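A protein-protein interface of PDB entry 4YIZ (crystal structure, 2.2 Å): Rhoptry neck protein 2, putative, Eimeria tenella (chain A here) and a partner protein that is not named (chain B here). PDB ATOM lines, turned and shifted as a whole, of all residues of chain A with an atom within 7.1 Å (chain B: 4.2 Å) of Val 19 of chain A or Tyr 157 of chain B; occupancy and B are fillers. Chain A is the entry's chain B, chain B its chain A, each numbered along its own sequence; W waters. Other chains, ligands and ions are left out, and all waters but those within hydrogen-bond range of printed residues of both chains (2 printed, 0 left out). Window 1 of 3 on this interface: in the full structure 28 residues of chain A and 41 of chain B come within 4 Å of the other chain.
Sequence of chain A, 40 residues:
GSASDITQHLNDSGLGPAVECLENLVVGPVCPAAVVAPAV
Water W1 lies within hydrogen-bond range of OH of Tyr 155 of chain B (2.6 Å) and N of Gly 16 of chain A (3.4 Å).
Water W2 lies within hydrogen-bond range of the side-chain hydroxyl (OH) of Tyr 157 of chain B (2.7 Å) and the backbone carbonyl oxygen (O) of Pro 17 of chain A (2.7 Å).
Among the printed residues, pairs that only touch across the chains: Gly 16 of chain A with Tyr 155 of chain B (3.7 Å), Pro 17 of chain A with Tyr 155 of chain B (3.7 Å), Pro 17 of chain A with Tyr 172 of chain B (3.8 Å), Val 19 of chain A with Phe 105 of chain B (3.9 Å), Val 19 of chain A with Ala 145 of chain B (3.99 Å), Val 19 of chain A with Met 146 of chain B (3.7 Å), Val 19 of chain A with Tyr 157 of chain B (3.3 Å), Val 19 of chain A with Tyr 172 of chain B (3.9 Å), Cys 21 of chain A with Ala 145 of chain B (3.96 Å), Leu 22 of chain A with Phe 105 of chain B (3.8 Å), Leu 22 of chain A with Tyr 157 of chain B (3.7 Å) and Pro 32 of chain A with Phe 105 of chain B (3.6 Å).
Of the printed residues of chain B, Val 19 of chain A touches Phe 105, Ala 145, Met 146, Tyr 157 and Tyr 172.
Of chain A, only Val 19 (3.3 Å) and Leu 22 (3.7 Å) come within 4 Å of Tyr 157 of chain B.
Printed residues of chain A within 4 Å of Tyr 172 of chain B: Pro 17 (3.8 Å) and Val 19 (3.9 Å).
Of the printed residues of chain A, Phe 105 of chain B touches Val 19 (3.9 Å), Leu 22 (3.8 Å) and Pro 32 (3.6 Å).
Pro 158 of chain B touches none of the printed residues of chain A.
Ile 170 of chain B touches none of the printed residues of chain A.
The nearest printed residue of chain A that does not touch Ala 145 of chain B is Leu 22 of chain A (4.01 Å).
The backbone NH (N) of Met 146 of chain B lies within hydrogen-bond range of the backbone carbonyl oxygen (O) of Cys 21 of chain A (2.9 Å).
The backbone carbonyl oxygen (O) of Tyr 155 of chain B is in hydrogen-bond range of the backbone NH (N) of Ala 145 of chain B.
Of the 9 printed residues of chain A, 6 touch a printed residue of chain B.
Hydrophobic or aromatic side chains of chain A that line the printed part of chain B: Pro 17, Val 19, Leu 22 and Pro 32.
Printed residues of chain B that touch a printed residue of chain A: Phe 105, Ala 145, Met 146, Tyr 155, Tyr 157 and Tyr 172.
Hydrophobic or aromatic side chains of chain B that line the printed part of chain A: Phe 105, Ala 145, Met 146, Tyr 155, Tyr 157 and Tyr 172.
Among the printed residues, 13 pairs touch across the chains.
Among the printed residues, no Asp or Glu carboxylate lies within 4 Å of a Lys or Arg side-chain nitrogen of the other chain.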
ATOM      1  N   GLY A  16      31.090 -11.310 -26.420  1.00  0.00           N
ATOM      2  CA  GLY A  16      30.905 -10.007 -27.029  1.00  0.00           C
ATOM      3  C   GLY A  16      32.112  -9.096 -26.927  1.00  0.00           C
ATOM      4  O   GLY A  16      33.096  -9.433 -26.267  1.00  0.00           O
ATOM      5  N   PRO A  17      32.040  -7.932 -27.588  1.00  0.00           N
ATOM      6  CA  PRO A  17      33.113  -6.932 -27.556  1.00  0.00           C
ATOM      7  C   PRO A  17      33.208  -6.208 -26.222  1.00  0.00           C
ATOM      8  O   PRO A  17      32.192  -5.997 -25.561  1.00  0.00           O
ATOM      9  CB  PRO A  17      32.714  -5.955 -28.666  1.00  0.00           C
ATOM     10  CG  PRO A  17      31.240  -6.090 -28.783  1.00  0.00           C
ATOM     11  CD  PRO A  17      30.926  -7.521 -28.462  1.00  0.00           C
ATOM     12  N   ALA A  18      34.424  -5.837 -25.836  1.00  0.00           N
ATOM     13  CA  ALA A  18      34.627  -4.991 -24.668  1.00  0.00           C
ATOM     14  C   ALA A  18      34.204  -3.566 -24.995  1.00  0.00           C
ATOM     15  O   ALA A  18      34.927  -2.840 -25.678  1.00  0.00           O
ATOM     16  CB  ALA A  18      36.076  -5.030 -24.225  1.00  0.00           C
ATOM     17  N   VAL A  19      33.028  -3.176 -24.509  1.00  0.00           N
ATOM     18  CA  VAL A  19      32.497  -1.841 -24.756  1.00  0.00           C
ATOM     19  C   VAL A  19      32.382  -1.054 -23.459  1.00  0.00           C
ATOM     20  O   VAL A  19      32.108  -1.615 -22.398  1.00  0.00           O
ATOM     21  CB  VAL A  19      31.117  -1.891 -25.441  1.00  0.00           C
ATOM     22  CG1 VAL A  19      31.244  -2.500 -26.824  1.00  0.00           C
ATOM     23  CG2 VAL A  19      30.113  -2.668 -24.597  1.00  0.00           C
ATOM     24  N   GLU A  20      32.600   0.251 -23.566  1.00  0.00           N
ATOM     25  CA  GLU A  20      32.533   1.152 -22.425  1.00  0.00           C
ATOM     26  C   GLU A  20      31.163   1.803 -22.311  1.00  0.00           C
ATOM     27  O   GLU A  20      30.762   2.224 -21.226  1.00  0.00           O
ATOM     28  CB  GLU A  20      33.616   2.233 -22.546  1.00  0.00           C
ATOM     29  CG  GLU A  20      33.575   3.320 -21.467  1.00  0.00           C
ATOM     30  CD  GLU A  20      33.808   2.776 -20.069  1.00  0.00           C
ATOM     31  OE1 GLU A  20      34.609   1.829 -19.925  1.00  0.00           O
ATOM     32  OE2 GLU A  20      33.191   3.297 -19.114  1.00  0.00           O
ATOM     33  N   CYS A  21      30.443   1.862 -23.430  1.00  0.00           N
ATOM     34  CA  CYS A  21      29.207   2.630 -23.511  1.00  0.00           C
ATOM     35  C   CYS A  21      28.162   1.976 -24.410  1.00  0.00           C
ATOM     36  O   CYS A  21      28.492   1.432 -25.465  1.00  0.00           O
ATOM     37  CB  CYS A  21      29.509   4.038 -24.027  1.00  0.00           C
ATOM     38  SG  CYS A  21      28.059   5.100 -24.213  1.00  0.00           S
ATOM     39  N   LEU A  22      26.903   2.041 -23.980  1.00  0.00           N
ATOM     40  CA  LEU A  22      25.772   1.644 -24.815  1.00  0.00           C
ATOM     41  C   LEU A  22      24.895   2.871 -25.032  1.00  0.00           C
ATOM     42  O   LEU A  22      24.763   3.701 -24.136  1.00  0.00           O
ATOM     43  CB  LEU A  22      24.965   0.510 -24.170  1.00  0.00           C
ATOM     44  CG  LEU A  22      25.288  -0.930 -24.582  1.00  0.00           C
ATOM     45  CD1 LEU A  22      26.774  -1.223 -24.524  1.00  0.00           C
ATOM     46  CD2 LEU A  22      24.529  -1.895 -23.690  1.00  0.00           C
ATOM     47  N   PRO A  32      29.092   1.607 -17.389  1.00  0.00           N
ATOM     48  CA  PRO A  32      29.237   0.980 -16.074  1.00  0.00           C
ATOM     49  C   PRO A  32      29.885   1.932 -15.072  1.00  0.00           C
ATOM     50  O   PRO A  32      30.858   2.604 -15.413  1.00  0.00           O
ATOM     51  CB  PRO A  32      30.131  -0.224 -16.361  1.00  0.00           C
ATOM     52  CG  PRO A  32      30.970   0.209 -17.518  1.00  0.00           C
ATOM     53  CD  PRO A  32      30.101   1.121 -18.349  1.00  0.00           C
ATOM     54  N   VAL A  36      33.897  -3.372 -15.270  1.00  0.00           N
ATOM     55  CA  VAL A  36      33.365  -4.721 -15.408  1.00  0.00           C
ATOM     56  C   VAL A  36      34.521  -5.710 -15.502  1.00  0.00           C
ATOM     57  O   VAL A  36      35.574  -5.387 -16.050  1.00  0.00           O
ATOM     58  CB  VAL A  36      32.462  -4.848 -16.660  1.00  0.00           C
ATOM     59  CG1 VAL A  36      31.940  -6.274 -16.825  1.00  0.00           C
ATOM     60  CG2 VAL A  36      31.302  -3.871 -16.577  1.00  0.00           C
ATOM     61  N   PHE B 105      24.924  -1.405 -16.681  1.00  0.00           N
ATOM     62  CA  PHE B 105      25.271  -0.027 -17.022  1.00  0.00           C
ATOM     63  C   PHE B 105      24.207   0.941 -16.510  1.00  0.00           C
ATOM     64  O   PHE B 105      23.050   0.564 -16.336  1.00  0.00           O
ATOM     65  CB  PHE B 105      25.433   0.144 -18.536  1.00  0.00           C
ATOM     66  CG  PHE B 105      26.627  -0.572 -19.120  1.00  0.00           C
ATOM     67  CD1 PHE B 105      27.340  -1.508 -18.386  1.00  0.00           C
ATOM     68  CD2 PHE B 105      27.037  -0.296 -20.413  1.00  0.00           C
ATOM     69  CE1 PHE B 105      28.430  -2.155 -18.934  1.00  0.00           C
ATOM     70  CE2 PHE B 105      28.127  -0.939 -20.965  1.00  0.00           C
ATOM     71  CZ  PHE B 105      28.823  -1.870 -20.225  1.00  0.00           C
ATOM     72  N   ALA B 145      25.580  -0.978 -29.037  1.00  0.00           N
ATOM     73  CA  ALA B 145      26.919  -0.775 -28.510  1.00  0.00           C
ATOM     74  C   ALA B 145      27.586   0.421 -29.180  1.00  0.00           C
ATOM     75  O   ALA B 145      27.432   0.633 -30.383  1.00  0.00           O
ATOM     76  CB  ALA B 145      27.757  -2.025 -28.712  1.00  0.00           C
ATOM     77  N   MET B 146      28.317   1.201 -28.389  1.00  0.00           N
ATOM     78  CA  MET B 146      29.164   2.267 -28.915  1.00  0.00           C
ATOM     79  C   MET B 146      30.586   1.735 -29.055  1.00  0.00           C
ATOM     80  O   MET B 146      31.033   0.935 -28.232  1.00  0.00           O
ATOM     81  CB  MET B 146      29.141   3.494 -27.998  1.00  0.00           C
ATOM     82  CG  MET B 146      27.759   4.098 -27.788  1.00  0.00           C
ATOM     83  SD  MET B 146      27.017   4.733 -29.305  1.00  0.00           S
ATOM     84  CE  MET B 146      27.223   6.499 -29.080  1.00  0.00           C
ATOM     85  N   TYR B 155      25.589  -3.525 -33.340  1.00  0.00           N
ATOM     86  CA  TYR B 155      25.625  -4.678 -32.453  1.00  0.00           C
ATOM     87  C   TYR B 155      24.612  -4.488 -31.331  1.00  0.00           C
ATOM     88  O   TYR B 155      24.665  -3.503 -30.594  1.00  0.00           O
ATOM     89  CB  TYR B 155      27.029  -4.873 -31.884  1.00  0.00           C
ATOM     90  CG  TYR B 155      27.171  -6.085 -30.991  1.00  0.00           C
ATOM     91  CD1 TYR B 155      26.933  -5.997 -29.627  1.00  0.00           C
ATOM     92  CD2 TYR B 155      27.549  -7.314 -31.511  1.00  0.00           C
ATOM     93  CE1 TYR B 155      27.061  -7.099 -28.807  1.00  0.00           C
ATOM     94  CE2 TYR B 155      27.682  -8.425 -30.698  1.00  0.00           C
ATOM     95  CZ  TYR B 155      27.438  -8.309 -29.346  1.00  0.00           C
ATOM     96  OH  TYR B 155      27.567  -9.408 -28.527  1.00  0.00           O
ATOM     97  N   ARG B 156      23.686  -5.436 -31.215  1.00  0.00           N
ATOM     98  CA  ARG B 156      22.613  -5.354 -30.233  1.00  0.00           C
ATOM     99  C   ARG B 156      22.617  -6.566 -29.314  1.00  0.00           C
ATOM    100  O   ARG B 156      23.111  -7.635 -29.676  1.00  0.00           O
ATOM    101  CB  ARG B 156      21.259  -5.232 -30.930  1.00  0.00           C
ATOM    102  CG  ARG B 156      21.109  -3.972 -31.762  1.00  0.00           C
ATOM    103  CD  ARG B 156      19.718  -3.881 -32.351  1.00  0.00           C
ATOM    104  NE  ARG B 156      19.459  -2.588 -32.978  1.00  0.00           N
ATOM    105  CZ  ARG B 156      19.898  -2.234 -34.182  1.00  0.00           C
ATOM    106  NH1 ARG B 156      20.636  -3.068 -34.902  1.00  0.00           N
ATOM    107  NH2 ARG B 156      19.601  -1.036 -34.664  1.00  0.00           N
ATOM    108  N   TYR B 157      22.047  -6.385 -28.130  1.00  0.00           N
ATOM    109  CA  TYR B 157      22.075  -7.401 -27.091  1.00  0.00           C
ATOM    110  C   TYR B 157      20.720  -8.082 -26.959  1.00  0.00           C
ATOM    111  O   TYR B 157      19.688  -7.452 -27.174  1.00  0.00           O
ATOM    112  CB  TYR B 157      22.482  -6.771 -25.759  1.00  0.00           C
ATOM    113  CG  TYR B 157      23.877  -6.196 -25.782  1.00  0.00           C
ATOM    114  CD1 TYR B 157      24.107  -4.905 -26.239  1.00  0.00           C
ATOM    115  CD2 TYR B 157      24.968  -6.946 -25.363  1.00  0.00           C
ATOM    116  CE1 TYR B 157      25.381  -4.376 -26.271  1.00  0.00           C
ATOM    117  CE2 TYR B 157      26.248  -6.424 -25.391  1.00  0.00           C
ATOM    118  CZ  TYR B 157      26.446  -5.137 -25.846  1.00  0.00           C
ATOM    119  OH  TYR B 157      27.717  -4.609 -25.878  1.00  0.00           O
ATOM    120  N   PRO B 158      20.714  -9.374 -26.602  1.00  0.00           N
ATOM    121  CA  PRO B 158      19.435 -10.061 -26.406  1.00  0.00           C
ATOM    122  C   PRO B 158      18.740  -9.604 -25.131  1.00  0.00           C
ATOM    123  O   PRO B 158      19.366  -8.967 -24.283  1.00  0.00           O
ATOM    124  CB  PRO B 158      19.837 -11.533 -26.315  1.00  0.00           C
ATOM    125  CG  PRO B 158      21.224 -11.505 -25.787  1.00  0.00           C
ATOM    126  CD  PRO B 158      21.862 -10.265 -26.352  1.00  0.00           C
ATOM    127  N   PHE B 159      17.462  -9.933 -25.007  1.00  0.00           N
ATOM    128  CA  PHE B 159      16.669  -9.522 -23.864  1.00  0.00           C
ATOM    129  C   PHE B 159      15.941 -10.704 -23.241  1.00  0.00           C
ATOM    130  O   PHE B 159      15.744 -11.749 -23.879  1.00  0.00           O
ATOM    131  CB  PHE B 159      15.651  -8.454 -24.278  1.00  0.00           C
ATOM    132  CG  PHE B 159      14.494  -9.001 -25.058  1.00  0.00           C
ATOM    133  CD1 PHE B 159      13.359  -9.454 -24.408  1.00  0.00           C
ATOM    134  CD2 PHE B 159      14.544  -9.070 -26.439  1.00  0.00           C
ATOM    135  CE1 PHE B 159      12.295  -9.967 -25.121  1.00  0.00           C
ATOM    136  CE2 PHE B 159      13.481  -9.578 -27.156  1.00  0.00           C
ATOM    137  CZ  PHE B 159      12.354 -10.028 -26.496  1.00  0.00           C
ATOM    138  N   ILE B 170      17.984  -6.521 -20.331  1.00  0.00           N
ATOM    139  CA  ILE B 170      18.957  -6.578 -21.416  1.00  0.00           C
ATOM    140  C   ILE B 170      20.158  -7.374 -20.918  1.00  0.00           C
ATOM    141  O   ILE B 170      20.708  -7.065 -19.863  1.00  0.00           O
ATOM    142  CB  ILE B 170      19.435  -5.180 -21.861  1.00  0.00           C
ATOM    143  CG1 ILE B 170      18.252  -4.253 -22.169  1.00  0.00           C
ATOM    144  CG2 ILE B 170      20.374  -5.296 -23.061  1.00  0.00           C
ATOM    145  CD1 ILE B 170      17.536  -4.549 -23.453  1.00  0.00           C
ATOM    146  N   LEU B 171      20.565  -8.391 -21.671  1.00  0.00           N
ATOM    147  CA  LEU B 171      21.698  -9.226 -21.278  1.00  0.00           C
ATOM    148  C   LEU B 171      22.997  -8.747 -21.908  1.00  0.00           C
ATOM    149  O   LEU B 171      23.112  -8.672 -23.128  1.00  0.00           O
ATOM    150  CB  LEU B 171      21.455 -10.682 -21.669  1.00  0.00           C
ATOM    151  CG  LEU B 171      20.206 -11.366 -21.114  1.00  0.00           C
ATOM    152  CD1 LEU B 171      20.244 -12.846 -21.458  1.00  0.00           C
ATOM    153  CD2 LEU B 171      20.082 -11.168 -19.615  1.00  0.00           C
ATOM    154  N   TYR B 172      23.980  -8.437 -21.072  1.00  0.00           N
ATOM    155  CA  TYR B 172      25.296  -8.044 -21.557  1.00  0.00           C
ATOM    156  C   TYR B 172      26.004  -9.241 -22.190  1.00  0.00           C
ATOM    157  O   TYR B 172      26.778  -9.091 -23.134  1.00  0.00           O
ATOM    158  CB  TYR B 172      26.129  -7.464 -20.414  1.00  0.00           C
ATOM    159  CG  TYR B 172      27.487  -6.937 -20.823  1.00  0.00           C
ATOM    160  CD1 TYR B 172      27.605  -5.800 -21.612  1.00  0.00           C
ATOM    161  CD2 TYR B 172      28.651  -7.564 -20.399  1.00  0.00           C
ATOM    162  CE1 TYR B 172      28.846  -5.311 -21.981  1.00  0.00           C
ATOM    163  CE2 TYR B 172      29.897  -7.081 -20.760  1.00  0.00           C
ATOM    164  CZ  TYR B 172      29.988  -5.954 -21.550  1.00  0.00           C
ATOM    165  OH  TYR B 172      31.224  -5.470 -21.913  1.00  0.00           O
ATOM    166  N   ALA B 215      17.460  -9.005 -29.935  1.00  0.00           N
ATOM    167  CA  ALA B 215      16.952  -7.641 -30.014  1.00  0.00           C
ATOM    168  C   ALA B 215      16.022  -7.467 -31.215  1.00  0.00           C
ATOM    169  O   ALA B 215      15.142  -6.603 -31.219  1.00  0.00           O
ATOM    170  CB  ALA B 215      18.107  -6.653 -30.089  1.00  0.00           C
HETATM  171  O   HOH W   1      28.979 -11.549 -29.101  1.00  0.00           O
HETATM  172  O   HOH W   2      29.507  -6.551 -25.426  1.00  0.00           O
